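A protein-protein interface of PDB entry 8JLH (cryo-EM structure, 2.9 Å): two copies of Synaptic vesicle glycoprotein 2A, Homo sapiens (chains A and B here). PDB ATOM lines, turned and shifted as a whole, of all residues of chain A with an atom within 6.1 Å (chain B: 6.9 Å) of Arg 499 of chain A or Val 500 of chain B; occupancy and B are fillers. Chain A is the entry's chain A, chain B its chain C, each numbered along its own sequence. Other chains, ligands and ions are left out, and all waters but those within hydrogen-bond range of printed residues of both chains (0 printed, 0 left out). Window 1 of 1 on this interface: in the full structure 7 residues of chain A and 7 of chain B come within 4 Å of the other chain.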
ATOM      1  N   GLY A 497      21.609  -7.716  22.872  1.00  0.00           N
ATOM      2  CA  GLY A 497      21.001  -6.403  22.800  1.00  0.00           C
ATOM      3  C   GLY A 497      19.783  -6.323  23.689  1.00  0.00           C
ATOM      4  O   GLY A 497      18.804  -7.037  23.463  1.00  0.00           O
ATOM      5  N   GLU A 498      19.822  -5.465  24.701  1.00  0.00           N
ATOM      6  CA  GLU A 498      18.771  -5.485  25.705  1.00  0.00           C
ATOM      7  C   GLU A 498      18.758  -4.187  26.499  1.00  0.00           C
ATOM      8  O   GLU A 498      19.688  -3.917  27.263  1.00  0.00           O
ATOM      9  CB  GLU A 498      18.978  -6.692  26.617  1.00  0.00           C
ATOM     10  CG  GLU A 498      17.826  -7.027  27.510  1.00  0.00           C
ATOM     11  CD  GLU A 498      17.944  -8.419  28.093  1.00  0.00           C
ATOM     12  OE1 GLU A 498      17.964  -8.552  29.333  1.00  0.00           O
ATOM     13  OE2 GLU A 498      18.020  -9.385  27.308  1.00  0.00           O
ATOM     14  N   ARG A 499      17.720  -3.375  26.330  1.00  0.00           N
ATOM     15  CA  ARG A 499      17.593  -2.118  27.051  1.00  0.00           C
ATOM     16  C   ARG A 499      16.548  -2.257  28.144  1.00  0.00           C
ATOM     17  O   ARG A 499      15.405  -2.627  27.871  1.00  0.00           O
ATOM     18  CB  ARG A 499      17.212  -0.974  26.113  1.00  0.00           C
ATOM     19  CG  ARG A 499      18.329  -0.518  25.212  1.00  0.00           C
ATOM     20  CD  ARG A 499      17.906   0.683  24.398  1.00  0.00           C
ATOM     21  NE  ARG A 499      17.514   1.796  25.253  1.00  0.00           N
ATOM     22  CZ  ARG A 499      17.998   3.025  25.146  1.00  0.00           C
ATOM     23  NH1 ARG A 499      18.895   3.337  24.226  1.00  0.00           N
ATOM     24  NH2 ARG A 499      17.570   3.967  25.982  1.00  0.00           N
ATOM     25  N   VAL A 500      16.946  -1.968  29.377  1.00  0.00           N
ATOM     26  CA  VAL A 500      16.038  -1.959  30.514  1.00  0.00           C
ATOM     27  C   VAL A 500      16.312  -0.694  31.311  1.00  0.00           C
ATOM     28  O   VAL A 500      17.456  -0.436  31.695  1.00  0.00           O
ATOM     29  CB  VAL A 500      16.206  -3.210  31.397  1.00  0.00           C
ATOM     30  CG1 VAL A 500      15.299  -3.124  32.584  1.00  0.00           C
ATOM     31  CG2 VAL A 500      15.908  -4.470  30.607  1.00  0.00           C
ATOM     32  N   GLU A 501      15.270   0.098  31.556  1.00  0.00           N
ATOM     33  CA  GLU A 501      15.423   1.389  32.212  1.00  0.00           C
ATOM     34  C   GLU A 501      14.375   1.547  33.301  1.00  0.00           C
ATOM     35  O   GLU A 501      13.205   1.223  33.086  1.00  0.00           O
ATOM     36  CB  GLU A 501      15.297   2.534  31.206  1.00  0.00           C
ATOM     37  CG  GLU A 501      16.307   2.478  30.084  1.00  0.00           C
ATOM     38  CD  GLU A 501      16.462   3.804  29.389  1.00  0.00           C
ATOM     39  OE1 GLU A 501      15.783   4.769  29.794  1.00  0.00           O
ATOM     40  OE2 GLU A 501      17.263   3.887  28.437  1.00  0.00           O
ATOM     41  N   VAL A 503      13.728   0.040  36.123  1.00  0.00           N
ATOM     42  CA  VAL A 503      13.071  -1.197  36.532  1.00  0.00           C
ATOM     43  C   VAL A 503      13.760  -1.730  37.781  1.00  0.00           C
ATOM     44  O   VAL A 503      14.991  -1.806  37.828  1.00  0.00           O
ATOM     45  CB  VAL A 503      13.097  -2.253  35.412  1.00  0.00           C
ATOM     46  CG1 VAL A 503      12.365  -3.512  35.845  1.00  0.00           C
ATOM     47  CG2 VAL A 503      12.491  -1.702  34.142  1.00  0.00           C
ATOM     48  N   GLY A 517      23.996  -5.222  26.337  1.00  0.00           N
ATOM     49  CA  GLY A 517      22.856  -4.618  26.992  1.00  0.00           C
ATOM     50  C   GLY A 517      23.089  -3.163  27.349  1.00  0.00           C
ATOM     51  O   GLY A 517      24.199  -2.637  27.282  1.00  0.00           O
ATOM     52  N   GLN A 518      22.001  -2.499  27.737  1.00  0.00           N
ATOM     53  CA  GLN A 518      22.031  -1.096  28.152  1.00  0.00           C
ATOM     54  C   GLN A 518      21.062  -0.941  29.318  1.00  0.00           C
ATOM     55  O   GLN A 518      19.844  -0.995  29.129  1.00  0.00           O
ATOM     56  CB  GLN A 518      21.666  -0.166  27.005  1.00  0.00           C
ATOM     57  CG  GLN A 518      22.758   0.017  25.975  1.00  0.00           C
ATOM     58  CD  GLN A 518      22.780   1.415  25.402  1.00  0.00           C
ATOM     59  OE1 GLN A 518      21.734   2.011  25.151  1.00  0.00           O
ATOM     60  NE2 GLN A 518      23.977   1.951  25.193  1.00  0.00           N
ATOM     61  N   TYR A 519      21.600  -0.748  30.516  1.00  0.00           N
ATOM     62  CA  TYR A 519      20.801  -0.632  31.728  1.00  0.00           C
ATOM     63  C   TYR A 519      21.047   0.733  32.354  1.00  0.00           C
ATOM     64  O   TYR A 519      22.182   1.057  32.714  1.00  0.00           O
ATOM     65  CB  TYR A 519      21.141  -1.759  32.704  1.00  0.00           C
ATOM     66  CG  TYR A 519      21.260  -3.100  32.020  1.00  0.00           C
ATOM     67  CD1 TYR A 519      22.488  -3.564  31.571  1.00  0.00           C
ATOM     68  CD2 TYR A 519      20.144  -3.889  31.797  1.00  0.00           C
ATOM     69  CE1 TYR A 519      22.601  -4.778  30.935  1.00  0.00           C
ATOM     70  CE2 TYR A 519      20.250  -5.108  31.160  1.00  0.00           C
ATOM     71  CZ  TYR A 519      21.480  -5.546  30.731  1.00  0.00           C
ATOM     72  OH  TYR A 519      21.593  -6.759  30.097  1.00  0.00           O
ATOM     73  N   GLU B 498       9.059   3.483  32.303  1.00  0.00           N
ATOM     74  CA  GLU B 498       9.738   2.198  32.371  1.00  0.00           C
ATOM     75  C   GLU B 498       9.984   1.704  30.955  1.00  0.00           C
ATOM     76  O   GLU B 498       9.030   1.447  30.216  1.00  0.00           O
ATOM     77  CB  GLU B 498       8.883   1.203  33.157  1.00  0.00           C
ATOM     78  CG  GLU B 498       9.637   0.271  34.058  1.00  0.00           C
ATOM     79  CD  GLU B 498       8.711  -0.588  34.888  1.00  0.00           C
ATOM     80  OE1 GLU B 498       9.204  -1.391  35.706  1.00  0.00           O
ATOM     81  OE2 GLU B 498       7.482  -0.453  34.727  1.00  0.00           O
ATOM     82  N   ARG B 499      11.251   1.576  30.572  1.00  0.00           N
ATOM     83  CA  ARG B 499      11.613   1.099  29.244  1.00  0.00           C
ATOM     84  C   ARG B 499      12.190  -0.303  29.326  1.00  0.00           C
ATOM     85  O   ARG B 499      13.115  -0.557  30.101  1.00  0.00           O
ATOM     86  CB  ARG B 499      12.621   2.022  28.566  1.00  0.00           C
ATOM     87  CG  ARG B 499      12.007   3.214  27.886  1.00  0.00           C
ATOM     88  CD  ARG B 499      13.065   4.001  27.153  1.00  0.00           C
ATOM     89  NE  ARG B 499      13.718   3.194  26.130  1.00  0.00           N
ATOM     90  CZ  ARG B 499      13.894   3.578  24.874  1.00  0.00           C
ATOM     91  NH1 ARG B 499      13.470   4.755  24.446  1.00  0.00           N
ATOM     92  NH2 ARG B 499      14.513   2.762  24.027  1.00  0.00           N
ATOM     93  N   VAL B 500      11.638  -1.208  28.525  1.00  0.00           N
ATOM     94  CA  VAL B 500      12.137  -2.571  28.391  1.00  0.00           C
ATOM     95  C   VAL B 500      12.154  -2.904  26.907  1.00  0.00           C
ATOM     96  O   VAL B 500      11.186  -2.618  26.198  1.00  0.00           O
ATOM     97  CB  VAL B 500      11.271  -3.576  29.173  1.00  0.00           C
ATOM     98  CG1 VAL B 500      11.766  -4.971  28.951  1.00  0.00           C
ATOM     99  CG2 VAL B 500      11.278  -3.253  30.654  1.00  0.00           C
ATOM    100  N   GLU B 501      13.260  -3.467  26.425  1.00  0.00           N
ATOM    101  CA  GLU B 501      13.403  -3.798  25.011  1.00  0.00           C
ATOM    102  C   GLU B 501      14.112  -5.134  24.860  1.00  0.00           C
ATOM    103  O   GLU B 501      15.108  -5.388  25.541  1.00  0.00           O
ATOM    104  CB  GLU B 501      14.181  -2.716  24.254  1.00  0.00           C
ATOM    105  CG  GLU B 501      13.846  -1.295  24.650  1.00  0.00           C
ATOM    106  CD  GLU B 501      13.646  -0.396  23.456  1.00  0.00           C
ATOM    107  OE1 GLU B 501      14.417  -0.522  22.484  1.00  0.00           O
ATOM    108  OE2 GLU B 501      12.715   0.434  23.488  1.00  0.00           O
ATOM    109  N   HIS B 502      13.599  -5.973  23.958  1.00  0.00           N
ATOM    110  CA  HIS B 502      14.216  -7.253  23.600  1.00  0.00           C
ATOM    111  C   HIS B 502      14.408  -8.165  24.812  1.00  0.00           C
ATOM    112  O   HIS B 502      15.440  -8.820  24.944  1.00  0.00           O
ATOM    113  CB  HIS B 502      15.551  -7.041  22.883  1.00  0.00           C
ATOM    114  CG  HIS B 502      15.444  -6.243  21.621  1.00  0.00           C
ATOM    115  ND1 HIS B 502      16.005  -4.993  21.483  1.00  0.00           N
ATOM    116  CD2 HIS B 502      14.851  -6.521  20.437  1.00  0.00           C
ATOM    117  CE1 HIS B 502      15.754  -4.531  20.272  1.00  0.00           C
ATOM    118  NE2 HIS B 502      15.056  -5.440  19.617  1.00  0.00           N
ATOM    119  N   VAL B 503      13.412  -8.227  25.692  1.00  0.00           N
ATOM    120  CA  VAL B 503      13.488  -9.018  26.916  1.00  0.00           C
ATOM    121  C   VAL B 503      12.379 -10.059  26.901  1.00  0.00           C
ATOM    122  O   VAL B 503      11.257  -9.772  26.469  1.00  0.00           O
ATOM    123  CB  VAL B 503      13.382  -8.133  28.171  1.00  0.00           C
ATOM    124  CG1 VAL B 503      13.468  -8.972  29.434  1.00  0.00           C
ATOM    125  CG2 VAL B 503      14.461  -7.086  28.171  1.00  0.00           C
ATOM    126  N   THR B 504      12.696 -11.268  27.357  1.00  0.00           N
ATOM    127  CA  THR B 504      11.691 -12.294  27.588  1.00  0.00           C
ATOM    128  C   THR B 504      11.286 -12.303  29.058  1.00  0.00           C
ATOM    129  O   THR B 504      12.094 -12.024  29.946  1.00  0.00           O
ATOM    130  CB  THR B 504      12.221 -13.668  27.175  1.00  0.00           C
ATOM    131  OG1 THR B 504      12.878 -13.563  25.907  1.00  0.00           O
ATOM    132  CG2 THR B 504      11.085 -14.667  27.058  1.00  0.00           C
ATOM    133  N   PHE B 505      10.017 -12.620  29.311  1.00  0.00           N
ATOM    134  CA  PHE B 505       9.442 -12.447  30.636  1.00  0.00           C
ATOM    135  C   PHE B 505       8.556 -13.625  31.015  1.00  0.00           C
ATOM    136  O   PHE B 505       7.747 -14.105  30.218  1.00  0.00           O
ATOM    137  CB  PHE B 505       8.588 -11.177  30.714  1.00  0.00           C
ATOM    138  CG  PHE B 505       9.373  -9.912  30.881  1.00  0.00           C
ATOM    139  CD1 PHE B 505      10.107  -9.678  32.029  1.00  0.00           C
ATOM    140  CD2 PHE B 505       9.346  -8.939  29.900  1.00  0.00           C
ATOM    141  CE1 PHE B 505      10.814  -8.506  32.185  1.00  0.00           C
ATOM    142  CE2 PHE B 505      10.047  -7.769  30.050  1.00  0.00           C
ATOM    143  CZ  PHE B 505      10.784  -7.550  31.194  1.00  0.00           C
ATOM    144  N   GLY B 517       5.046   3.555  30.254  1.00  0.00           N
ATOM    145  CA  GLY B 517       6.049   2.599  29.839  1.00  0.00           C
ATOM    146  C   GLY B 517       6.277   2.612  28.341  1.00  0.00           C
ATOM    147  O   GLY B 517       5.522   3.198  27.567  1.00  0.00           O
ATOM    148  N   GLN B 518       7.354   1.948  27.925  1.00  0.00           N
ATOM    149  CA  GLN B 518       7.711   1.828  26.511  1.00  0.00           C
ATOM    150  C   GLN B 518       8.371   0.469  26.313  1.00  0.00           C
ATOM    151  O   GLN B 518       9.506   0.255  26.746  1.00  0.00           O
ATOM    152  CB  GLN B 518       8.633   2.955  26.068  1.00  0.00           C
ATOM    153  CG  GLN B 518       7.922   4.240  25.713  1.00  0.00           C
ATOM    154  CD  GLN B 518       8.532   4.912  24.506  1.00  0.00           C
ATOM    155  OE1 GLN B 518       9.745   4.877  24.311  1.00  0.00           O
ATOM    156  NE2 GLN B 518       7.691   5.530  23.685  1.00  0.00           N
ATOM    157  N   TYR B 519       7.660  -0.442  25.657  1.00  0.00           N
ATOM    158  CA  TYR B 519       8.133  -1.803  25.440  1.00  0.00           C
ATOM    159  C   TYR B 519       8.249  -2.050  23.942  1.00  0.00           C
ATOM    160  O   TYR B 519       7.297  -1.807  23.197  1.00  0.00           O
ATOM    161  CB  TYR B 519       7.187  -2.809  26.093  1.00  0.00           C
ATOM    162  CG  TYR B 519       6.748  -2.391  27.477  1.00  0.00           C
ATOM    163  CD1 TYR B 519       5.570  -1.688  27.669  1.00  0.00           C
ATOM    164  CD2 TYR B 519       7.523  -2.679  28.589  1.00  0.00           C
ATOM    165  CE1 TYR B 519       5.169  -1.295  28.926  1.00  0.00           C
ATOM    166  CE2 TYR B 519       7.130  -2.289  29.852  1.00  0.00           C
ATOM    167  CZ  TYR B 519       5.951  -1.597  30.013  1.00  0.00           C
ATOM    168  OH  TYR B 519       5.554  -1.207  31.268  1.00  0.00           O
ATOM    169  N   PHE B 520       9.416  -2.517  23.503  1.00  0.00           N
ATOM    170  CA  PHE B 520       9.675  -2.777  22.090  1.00  0.00           C
ATOM    171  C   PHE B 520      10.233  -4.183  21.926  1.00  0.00           C
ATOM    172  O   PHE B 520      11.254  -4.525  22.530  1.00  0.00           O
ATOM    173  CB  PHE B 520      10.631  -1.739  21.504  1.00  0.00           C
ATOM    174  CG  PHE B 520      10.914  -1.936  20.040  1.00  0.00           C
ATOM    175  CD1 PHE B 520      10.167  -1.276  19.083  1.00  0.00           C
ATOM    176  CD2 PHE B 520      11.938  -2.768  19.622  1.00  0.00           C
ATOM    177  CE1 PHE B 520      10.423  -1.456  17.739  1.00  0.00           C
ATOM    178  CE2 PHE B 520      12.197  -2.951  18.280  1.00  0.00           C
ATOM    179  CZ  PHE B 520      11.441  -2.293  17.340  1.00  0.00           C
ATOM    180  N   ASN B 521       9.563  -4.984  21.098  1.00  0.00           N
ATOM    181  CA  ASN B 521      10.016  -6.317  20.703  1.00  0.00           C
ATOM    182  C   ASN B 521      10.235  -7.220  21.918  1.00  0.00           C
ATOM    183  O   ASN B 521      11.160  -8.029  21.970  1.00  0.00           O
ATOM    184  CB  ASN B 521      11.282  -6.223  19.848  1.00  0.00           C
ATOM    185  CG  ASN B 521      11.373  -7.327  18.822  1.00  0.00           C
ATOM    186  OD1 ASN B 521      11.421  -8.507  19.165  1.00  0.00           O
ATOM    187  ND2 ASN B 521      11.392  -6.950  17.551  1.00  0.00           N
ATOM    188  N   ASP B 522       9.349  -7.078  22.897  1.00  0.00           N
ATOM    189  CA  ASP B 522       9.383  -7.874  24.113  1.00  0.00           C
ATOM    190  C   ASP B 522       8.469  -9.075  23.963  1.00  0.00           C
ATOM    191  O   ASP B 522       7.406  -8.982  23.346  1.00  0.00           O
ATOM    192  CB  ASP B 522       8.950  -7.059  25.326  1.00  0.00           C
ATOM    193  CG  ASP B 522       9.996  -6.076  25.770  1.00  0.00           C
ATOM    194  OD1 ASP B 522      11.092  -6.512  26.164  1.00  0.00           O
ATOM    195  OD2 ASP B 522       9.719  -4.865  25.731  1.00  0.00           O
ATOM    196  N   PHE B 524       6.293 -11.698  26.208  1.00  0.00           N
ATOM    197  CA  PHE B 524       5.677 -11.869  27.517  1.00  0.00           C
ATOM    198  C   PHE B 524       5.011 -13.241  27.513  1.00  0.00           C
ATOM    199  O   PHE B 524       3.867 -13.376  27.074  1.00  0.00           O
ATOM    200  CB  PHE B 524       4.665 -10.759  27.789  1.00  0.00           C
ATOM    201  CG  PHE B 524       5.236  -9.373  27.721  1.00  0.00           C
ATOM    202  CD1 PHE B 524       5.975  -8.858  28.767  1.00  0.00           C
ATOM    203  CD2 PHE B 524       5.010  -8.576  26.616  1.00  0.00           C
ATOM    204  CE1 PHE B 524       6.490  -7.582  28.703  1.00  0.00           C
ATOM    205  CE2 PHE B 524       5.522  -7.301  26.549  1.00  0.00           C
ATOM    206  CZ  PHE B 524       6.262  -6.805  27.596  1.00  0.00           C
ATOM    207  N   CYS B 542       5.416  -6.410  20.162  1.00  0.00           N
ATOM    208  CA  CYS B 542       5.529  -7.243  21.344  1.00  0.00           C
ATOM    209  C   CYS B 542       4.880  -8.599  21.090  1.00  0.00           C
ATOM    210  O   CYS B 542       4.339  -8.868  20.018  1.00  0.00           O
ATOM    211  CB  CYS B 542       4.911  -6.539  22.548  1.00  0.00           C
ATOM    212  SG  CYS B 542       6.027  -5.399  23.390  1.00  0.00           S
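O of Arg 499 of chain A sits at hydrogen-bond distance from N of Glu 501 of chain B (2.7 Å). The backbone NH of Glu 501 of chain A lies within hydrogen-bond range of the backbone carbonyl oxygen of Arg 499 of chain B, at 2.7 Å. The guanidinium group of Arg 499 of chain A sits close to the guanidinium group of Arg 499 of chain B (3.4 Å).
Arg 499 of chain A touches just these residues of chain B: Arg 499, Val 500 and Glu 501. Printed residues of chain A within 4 Å of Val 500 of chain B: Arg 499 (3.3 Å). Of the printed residues of chain B, Glu 501 of chain A touches Glu 498 and Arg 499. Of the printed residues of chain B, Val 503 of chain A touches Glu 498 (3.5 Å). Printed residues of chain A within 4 Å of Arg 499 of chain B: Arg 499, Val 500 and Glu 501. Printed residues of chain B within 4 Å of Val 500 of chain A: Arg 499 (3.3 Å) and Val 503 (3.9 Å).
Glu 498 of chain A touches Val 503 of chain B, and with the chains exchanged Val 503 of chain A touches Glu 498 of chain B. Arg 499 of chain B touches its own counterpart, Arg 499 of chain A. Arg 499 of chain A touches Glu 501 of chain B, and with the chains exchanged Glu 501 of chain A touches Arg 499 of chain B. Val 500 of chain A touches Val 503 of chain B, but with the chains exchanged Val 503 of chain A does not touch Val 500 of chain B (4.01 Å). Of the 12 pairs that touch across the chains among the printed residues, 9 have their exchanged pair printed and touching as well.
The backbone NH of Gln 518 of chain A sits at hydrogen-bond distance from the backbone carbonyl oxygen of Glu 498 of chain A, 2.8 Å away. The guanidinium group (NH1) of Arg 499 of chain A is in hydrogen-bond range of the side-chain amide oxygen (OE1) of Gln 518 of chain A. The backbone NH of Val 500 of chain A lies within hydrogen-bond range of the backbone carbonyl oxygen of Gln 518 of chain A, at 3.1 Å. NH2 of Arg 499 of chain B is in salt-bridge range of OE2 of Glu 501 of chain B. The side-chain carboxylate (OD2) of Asp 522 of chain B sits close to the backbone carbonyl oxygen (O) of Val 500 of chain B (2.7 Å). The backbone NH (N) of His 502 of chain B is in hydrogen-bond range of the side-chain carboxylate (OD1) of Asp 522 of chain B.
Printed residues of chain B that touch a printed residue of chain A: Glu 498, Arg 499, Val 500, Glu 501, His 502 and Val 503. Among the printed residues, no Asp or Glu carboxylate lies within 4 Å of a Lys or Arg side-chain nitrogen of the other chain.
Among the printed residues, merely in contact across the chains: Gly 497 of chain A with His 502 of chain B (3.3 Å), Glu 498 of chain A with Glu 501 of chain B (3.7 Å), Glu 498 of chain A with His 502 of chain B (3.5 Å), Glu 498 of chain A with Val 503 of chain B (3.4 Å), Arg 499 of chain A with Val 500 of chain B (3.3 Å), Val 500 of chain A with Arg 499 of chain B (3.3 Å), Val 500 of chain A with Val 503 of chain B (3.9 Å), Glu 501 of chain A with Glu 498 of chain B (3.7 Å) and Val 503 of chain A with Glu 498 of chain B (3.5 Å).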
